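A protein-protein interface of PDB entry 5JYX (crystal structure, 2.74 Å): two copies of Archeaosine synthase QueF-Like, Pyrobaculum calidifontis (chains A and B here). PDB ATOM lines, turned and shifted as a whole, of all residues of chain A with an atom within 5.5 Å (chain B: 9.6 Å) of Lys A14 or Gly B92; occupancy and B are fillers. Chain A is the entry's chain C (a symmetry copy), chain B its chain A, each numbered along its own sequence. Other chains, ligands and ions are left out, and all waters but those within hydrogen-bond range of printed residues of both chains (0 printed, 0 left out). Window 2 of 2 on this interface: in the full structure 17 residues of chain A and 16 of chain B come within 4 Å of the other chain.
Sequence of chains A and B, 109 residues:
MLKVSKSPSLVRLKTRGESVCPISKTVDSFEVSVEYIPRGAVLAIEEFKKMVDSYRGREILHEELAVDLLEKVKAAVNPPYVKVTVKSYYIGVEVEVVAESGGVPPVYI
The backbone NH of Ser B88 lies within hydrogen-bond range of the backbone carbonyl oxygen of Val B95, 2.9 Å away. N of Leu A13 lies within hydrogen-bond range of O of Val A34 (2.9 Å). O of Thr A15 sits at hydrogen-bond distance from N of Val A32.
Glu B94 touches Arg A12. Arg A12 touches Val B95 (O to CA, 3.5 Å). Leu A13 touches Glu B94 (CA to O, 3.3 Å). O of Gly B92 touches O of Lys A14 (3.96 Å). CA of Val B93 touches O of Lys A14, at 3.4 Å. Phe A48 touches Val B93 (CD2 to CG1, 3.9 Å).
Printed residues of chain B that touch a printed residue of chain A: Gly B92, Val B93, Glu B94, Val B95 and Glu B96. Hydrophobic or aromatic side chains of chain B within 4 Å of the printed part of chain A: Val B93. Of the 10 printed residues of chain A, 5 touch a printed residue of chain B. Printed residues of chain A that touch a printed residue of chain B: Arg A12, Leu A13, Lys A14, Thr A15 and Phe A48. Hydrophobic or aromatic side chains of chain A that line the printed part of chain B: Phe A48. Along chain A the printed residues that touch a printed residue of chain B span positions 12 to 48. Among the printed residues, 9 pairs touch across the chains.
Printed residues of chain B within 4 Å of Lys A14: Gly B92 (3.96 Å), Val B93 (3.4 Å) and Glu B94 (2.7 Å). Printed residues of chain A within 4 Å of Gly B92: Lys A14 and Thr A15. Of the printed residues of chain A, Glu B96 touches Arg A12 (2.9 Å). Printed residues of chain A within 4 Å of Val B93: Lys A14 (3.4 Å) and Phe A48 (3.9 Å).
No position is printed for both chains. Of the 9 pairs that touch across the chains among the printed residues, none has its exchanged pair printed and touching as well.
OG1 of Thr A15 lies within hydrogen-bond range of O of Gly B92 (2.6 Å). The backbone NH (N) of Glu B94 lies within hydrogen-bond range of the backbone carbonyl oxygen (O) of Lys A14, 2.7 Å away. NH1 of Arg A12 lies within salt-bridge range of OE2 of Glu B96, at 3.0 Å.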
ATOM      1  N   ARG A  12      -1.045  10.406  16.292  1.00  0.00           N
ATOM      2  CA  ARG A  12      -0.764  11.661  16.973  1.00  0.00           C
ATOM      3  C   ARG A  12      -2.118  12.265  17.324  1.00  0.00           C
ATOM      4  O   ARG A  12      -3.059  12.213  16.522  1.00  0.00           O
ATOM      5  CB  ARG A  12       0.043  12.661  16.130  1.00  0.00           C
ATOM      6  CG  ARG A  12       1.260  12.081  15.427  1.00  0.00           C
ATOM      7  CD  ARG A  12       2.054  13.120  14.621  1.00  0.00           C
ATOM      8  NE  ARG A  12       3.230  12.551  13.927  1.00  0.00           N
ATOM      9  CZ  ARG A  12       3.233  11.853  12.774  1.00  0.00           C
ATOM     10  NH1 ARG A  12       2.122  11.546  12.085  1.00  0.00           N
ATOM     11  NH2 ARG A  12       4.388  11.416  12.302  1.00  0.00           N
ATOM     12  N   LEU A  13      -2.197  12.827  18.515  1.00  0.00           N
ATOM     13  CA  LEU A  13      -3.287  13.660  18.910  1.00  0.00           C
ATOM     14  C   LEU A  13      -2.737  14.996  19.382  1.00  0.00           C
ATOM     15  O   LEU A  13      -1.722  15.035  19.976  1.00  0.00           O
ATOM     16  CB  LEU A  13      -4.013  13.022  20.038  1.00  0.00           C
ATOM     17  CG  LEU A  13      -4.513  11.620  19.787  1.00  0.00           C
ATOM     18  CD1 LEU A  13      -5.037  11.095  21.106  1.00  0.00           C
ATOM     19  CD2 LEU A  13      -5.604  11.581  18.755  1.00  0.00           C
ATOM     20  N   LYS A  14      -3.403  16.092  19.075  1.00  0.00           N
ATOM     21  CA  LYS A  14      -2.925  17.384  19.419  1.00  0.00           C
ATOM     22  C   LYS A  14      -4.062  18.320  19.758  1.00  0.00           C
ATOM     23  O   LYS A  14      -5.067  18.376  19.061  1.00  0.00           O
ATOM     24  CB  LYS A  14      -2.154  17.937  18.271  1.00  0.00           C
ATOM     25  CG  LYS A  14      -1.585  19.324  18.515  1.00  0.00           C
ATOM     26  CD  LYS A  14      -1.397  20.003  17.182  1.00  0.00           C
ATOM     27  CE  LYS A  14      -0.016  20.614  17.018  1.00  0.00           C
ATOM     28  NZ  LYS A  14       0.390  20.444  15.574  1.00  0.00           N
ATOM     29  N   THR A  15      -3.869  19.084  20.823  1.00  0.00           N
ATOM     30  CA  THR A  15      -4.860  20.015  21.287  1.00  0.00           C
ATOM     31  C   THR A  15      -4.249  21.092  22.228  1.00  0.00           C
ATOM     32  O   THR A  15      -3.060  21.099  22.519  1.00  0.00           O
ATOM     33  CB  THR A  15      -5.998  19.216  21.974  1.00  0.00           C
ATOM     34  OG1 THR A  15      -7.182  20.019  22.124  1.00  0.00           O
ATOM     35  CG2 THR A  15      -5.539  18.711  23.344  1.00  0.00           C
ATOM     36  N   ARG A  16      -5.113  22.000  22.673  1.00  0.00           N
ATOM     37  CA  ARG A  16      -4.776  23.094  23.549  1.00  0.00           C
ATOM     38  C   ARG A  16      -5.285  22.836  24.954  1.00  0.00           C
ATOM     39  O   ARG A  16      -6.320  22.256  25.169  1.00  0.00           O
ATOM     40  CB  ARG A  16      -5.366  24.399  23.039  1.00  0.00           C
ATOM     41  CG  ARG A  16      -4.937  24.717  21.628  1.00  0.00           C
ATOM     42  CD  ARG A  16      -4.479  26.143  21.403  1.00  0.00           C
ATOM     43  NE  ARG A  16      -3.068  26.272  21.787  1.00  0.00           N
ATOM     44  CZ  ARG A  16      -2.541  27.281  22.483  1.00  0.00           C
ATOM     45  NH1 ARG A  16      -3.317  28.288  22.914  1.00  0.00           N
ATOM     46  NH2 ARG A  16      -1.231  27.283  22.782  1.00  0.00           N
ATOM     47  N   GLU A  31      -0.004  24.160  24.014  1.00  0.00           N
ATOM     48  CA  GLU A  31      -0.334  23.218  22.971  1.00  0.00           C
ATOM     49  C   GLU A  31       0.373  21.914  23.338  1.00  0.00           C
ATOM     50  O   GLU A  31       1.523  21.919  23.687  1.00  0.00           O
ATOM     51  CB  GLU A  31       0.169  23.811  21.646  1.00  0.00           C
ATOM     52  CG  GLU A  31      -0.234  23.116  20.344  1.00  0.00           C
ATOM     53  CD  GLU A  31       0.685  23.540  19.144  1.00  0.00           C
ATOM     54  OE1 GLU A  31       0.485  24.698  18.675  1.00  0.00           O
ATOM     55  OE2 GLU A  31       1.609  22.732  18.707  1.00  0.00           O
ATOM     56  N   VAL A  32      -0.311  20.796  23.204  1.00  0.00           N
ATOM     57  CA  VAL A  32       0.240  19.512  23.566  1.00  0.00           C
ATOM     58  C   VAL A  32      -0.052  18.443  22.517  1.00  0.00           C
ATOM     59  O   VAL A  32      -1.122  18.361  22.059  1.00  0.00           O
ATOM     60  CB  VAL A  32      -0.295  19.108  24.920  1.00  0.00           C
ATOM     61  CG1 VAL A  32      -1.790  18.927  24.911  1.00  0.00           C
ATOM     62  CG2 VAL A  32       0.315  17.801  25.386  1.00  0.00           C
ATOM     63  N   SER A  33       0.938  17.649  22.133  1.00  0.00           N
ATOM     64  CA  SER A  33       0.786  16.477  21.229  1.00  0.00           C
ATOM     65  C   SER A  33       1.226  15.248  21.960  1.00  0.00           C
ATOM     66  O   SER A  33       2.145  15.312  22.764  1.00  0.00           O
ATOM     67  CB  SER A  33       1.695  16.549  20.007  1.00  0.00           C
ATOM     68  OG  SER A  33       1.878  17.918  19.600  1.00  0.00           O
ATOM     69  N   VAL A  34       0.569  14.137  21.667  1.00  0.00           N
ATOM     70  CA  VAL A  34       0.975  12.835  22.088  1.00  0.00           C
ATOM     71  C   VAL A  34       1.053  12.003  20.818  1.00  0.00           C
ATOM     72  O   VAL A  34       0.095  11.917  20.052  1.00  0.00           O
ATOM     73  CB  VAL A  34      -0.087  12.249  22.967  1.00  0.00           C
ATOM     74  CG1 VAL A  34       0.160  10.777  23.284  1.00  0.00           C
ATOM     75  CG2 VAL A  34      -0.183  13.061  24.202  1.00  0.00           C
ATOM     76  N   PHE A  48      -8.552  11.568  25.960  1.00  0.00           N
ATOM     77  CA  PHE A  48      -7.384  12.402  25.837  1.00  0.00           C
ATOM     78  C   PHE A  48      -7.744  13.851  26.192  1.00  0.00           C
ATOM     79  O   PHE A  48      -7.089  14.512  26.990  1.00  0.00           O
ATOM     80  CB  PHE A  48      -6.816  12.263  24.432  1.00  0.00           C
ATOM     81  CG  PHE A  48      -5.757  13.267  24.115  1.00  0.00           C
ATOM     82  CD1 PHE A  48      -4.500  13.162  24.679  1.00  0.00           C
ATOM     83  CD2 PHE A  48      -6.006  14.331  23.231  1.00  0.00           C
ATOM     84  CE1 PHE A  48      -3.511  14.101  24.377  1.00  0.00           C
ATOM     85  CE2 PHE A  48      -5.015  15.285  22.936  1.00  0.00           C
ATOM     86  CZ  PHE A  48      -3.767  15.164  23.513  1.00  0.00           C
ATOM     87  N   ASP B  28     -17.572  13.404   9.901  1.00  0.00           N
ATOM     88  CA  ASP B  28     -16.166  13.712  10.232  1.00  0.00           C
ATOM     89  C   ASP B  28     -15.472  13.947   8.952  1.00  0.00           C
ATOM     90  O   ASP B  28     -15.415  13.047   8.178  1.00  0.00           O
ATOM     91  CB  ASP B  28     -15.508  12.496  10.885  1.00  0.00           C
ATOM     92  CG  ASP B  28     -15.646  12.485  12.425  1.00  0.00           C
ATOM     93  OD1 ASP B  28     -15.811  13.611  13.003  1.00  0.00           O
ATOM     94  OD2 ASP B  28     -15.576  11.371  13.047  1.00  0.00           O
ATOM     95  N   LYS B  87      -5.959  12.310   8.444  1.00  0.00           N
ATOM     96  CA  LYS B  87      -5.849  13.572   9.250  1.00  0.00           C
ATOM     97  C   LYS B  87      -7.204  14.164   9.505  1.00  0.00           C
ATOM     98  O   LYS B  87      -7.924  14.409   8.594  1.00  0.00           O
ATOM     99  CB  LYS B  87      -5.089  14.640   8.514  1.00  0.00           C
ATOM    100  CG  LYS B  87      -3.646  14.623   8.851  1.00  0.00           C
ATOM    101  CD  LYS B  87      -2.784  15.500   7.958  1.00  0.00           C
ATOM    102  CE  LYS B  87      -1.279  15.135   8.092  1.00  0.00           C
ATOM    103  NZ  LYS B  87      -0.410  15.774   7.041  1.00  0.00           N
ATOM    104  N   SER B  88      -7.526  14.480  10.740  1.00  0.00           N
ATOM    105  CA  SER B  88      -8.882  14.822  11.084  1.00  0.00           C
ATOM    106  C   SER B  88      -8.872  15.733  12.271  1.00  0.00           C
ATOM    107  O   SER B  88      -7.832  16.151  12.672  1.00  0.00           O
ATOM    108  CB  SER B  88      -9.629  13.542  11.369  1.00  0.00           C
ATOM    109  OG  SER B  88     -10.883  13.586  10.723  1.00  0.00           O
ATOM    110  N   TYR B  89     -10.037  16.056  12.813  1.00  0.00           N
ATOM    111  CA  TYR B  89     -10.202  17.131  13.801  1.00  0.00           C
ATOM    112  C   TYR B  89     -11.513  16.850  14.467  1.00  0.00           C
ATOM    113  O   TYR B  89     -12.487  16.892  13.794  1.00  0.00           O
ATOM    114  CB  TYR B  89     -10.218  18.531  13.164  1.00  0.00           C
ATOM    115  CG  TYR B  89     -10.289  19.693  14.171  1.00  0.00           C
ATOM    116  CD1 TYR B  89     -11.533  20.142  14.726  1.00  0.00           C
ATOM    117  CD2 TYR B  89      -9.152  20.382  14.547  1.00  0.00           C
ATOM    118  CE1 TYR B  89     -11.597  21.224  15.617  1.00  0.00           C
ATOM    119  CE2 TYR B  89      -9.217  21.430  15.455  1.00  0.00           C
ATOM    120  CZ  TYR B  89     -10.440  21.842  15.975  1.00  0.00           C
ATOM    121  OH  TYR B  89     -10.447  22.887  16.856  1.00  0.00           O
ATOM    122  N   TYR B  90     -11.522  16.519  15.755  1.00  0.00           N
ATOM    123  CA  TYR B  90     -12.719  16.235  16.516  1.00  0.00           C
ATOM    124  C   TYR B  90     -12.634  16.912  17.896  1.00  0.00           C
ATOM    125  O   TYR B  90     -11.678  16.735  18.656  1.00  0.00           O
ATOM    126  CB  TYR B  90     -12.965  14.719  16.655  1.00  0.00           C
ATOM    127  CG  TYR B  90     -14.339  14.355  17.201  1.00  0.00           C
ATOM    128  CD1 TYR B  90     -15.505  14.801  16.579  1.00  0.00           C
ATOM    129  CD2 TYR B  90     -14.460  13.537  18.332  1.00  0.00           C
ATOM    130  CE1 TYR B  90     -16.758  14.468  17.079  1.00  0.00           C
ATOM    131  CE2 TYR B  90     -15.688  13.180  18.862  1.00  0.00           C
ATOM    132  CZ  TYR B  90     -16.862  13.636  18.260  1.00  0.00           C
ATOM    133  OH  TYR B  90     -18.126  13.295  18.851  1.00  0.00           O
ATOM    134  N   ILE B  91     -13.639  17.737  18.165  1.00  0.00           N
ATOM    135  CA  ILE B  91     -13.838  18.363  19.412  1.00  0.00           C
ATOM    136  C   ILE B  91     -12.560  18.988  19.973  1.00  0.00           C
ATOM    137  O   ILE B  91     -12.240  18.887  21.195  1.00  0.00           O
ATOM    138  CB  ILE B  91     -14.579  17.402  20.376  1.00  0.00           C
ATOM    139  CG1 ILE B  91     -13.759  16.168  20.776  1.00  0.00           C
ATOM    140  CG2 ILE B  91     -15.901  16.959  19.736  1.00  0.00           C
ATOM    141  CD1 ILE B  91     -14.340  15.395  21.937  1.00  0.00           C
ATOM    142  N   GLY B  92     -11.866  19.691  19.070  1.00  0.00           N
ATOM    143  CA  GLY B  92     -10.736  20.551  19.421  1.00  0.00           C
ATOM    144  C   GLY B  92      -9.471  19.757  19.420  1.00  0.00           C
ATOM    145  O   GLY B  92      -8.471  20.225  19.891  1.00  0.00           O
ATOM    146  N   VAL B  93      -9.520  18.550  18.865  1.00  0.00           N
ATOM    147  CA  VAL B  93      -8.364  17.665  18.823  1.00  0.00           C
ATOM    148  C   VAL B  93      -7.931  17.425  17.408  1.00  0.00           C
ATOM    149  O   VAL B  93      -8.683  16.938  16.635  1.00  0.00           O
ATOM    150  CB  VAL B  93      -8.634  16.344  19.542  1.00  0.00           C
ATOM    151  CG1 VAL B  93      -7.338  15.609  19.743  1.00  0.00           C
ATOM    152  CG2 VAL B  93      -9.159  16.622  20.917  1.00  0.00           C
ATOM    153  N   GLU B  94      -6.706  17.769  17.067  1.00  0.00           N
ATOM    154  CA  GLU B  94      -6.131  17.327  15.770  1.00  0.00           C
ATOM    155  C   GLU B  94      -5.665  15.919  15.866  1.00  0.00           C
ATOM    156  O   GLU B  94      -5.066  15.575  16.837  1.00  0.00           O
ATOM    157  CB  GLU B  94      -4.958  18.159  15.398  1.00  0.00           C
ATOM    158  CG  GLU B  94      -5.425  19.465  14.865  1.00  0.00           C
ATOM    159  CD  GLU B  94      -4.259  20.354  14.645  1.00  0.00           C
ATOM    160  OE1 GLU B  94      -4.169  21.307  15.450  1.00  0.00           O
ATOM    161  OE2 GLU B  94      -3.421  20.062  13.720  1.00  0.00           O
ATOM    162  N   VAL B  95      -5.964  15.132  14.847  1.00  0.00           N
ATOM    163  CA  VAL B  95      -5.770  13.690  14.828  1.00  0.00           C
ATOM    164  C   VAL B  95      -4.991  13.298  13.605  1.00  0.00           C
ATOM    165  O   VAL B  95      -5.355  13.710  12.530  1.00  0.00           O
ATOM    166  CB  VAL B  95      -7.110  12.955  14.691  1.00  0.00           C
ATOM    167  CG1 VAL B  95      -6.885  11.466  14.503  1.00  0.00           C
ATOM    168  CG2 VAL B  95      -7.960  13.197  15.928  1.00  0.00           C
ATOM    169  N   GLU B  96      -3.944  12.485  13.782  1.00  0.00           N
ATOM    170  CA  GLU B  96      -3.311  11.768  12.656  1.00  0.00           C
ATOM    171  C   GLU B  96      -3.220  10.327  12.917  1.00  0.00           C
ATOM    172  O   GLU B  96      -2.849   9.947  13.973  1.00  0.00           O
ATOM    173  CB  GLU B  96      -1.918  12.255  12.412  1.00  0.00           C
ATOM    174  CG  GLU B  96      -1.944  13.715  12.092  1.00  0.00           C
ATOM    175  CD  GLU B  96      -0.649  14.230  11.494  1.00  0.00           C
ATOM    176  OE1 GLU B  96      -0.420  15.508  11.745  1.00  0.00           O
ATOM    177  OE2 GLU B  96       0.056  13.359  10.795  1.00  0.00           O
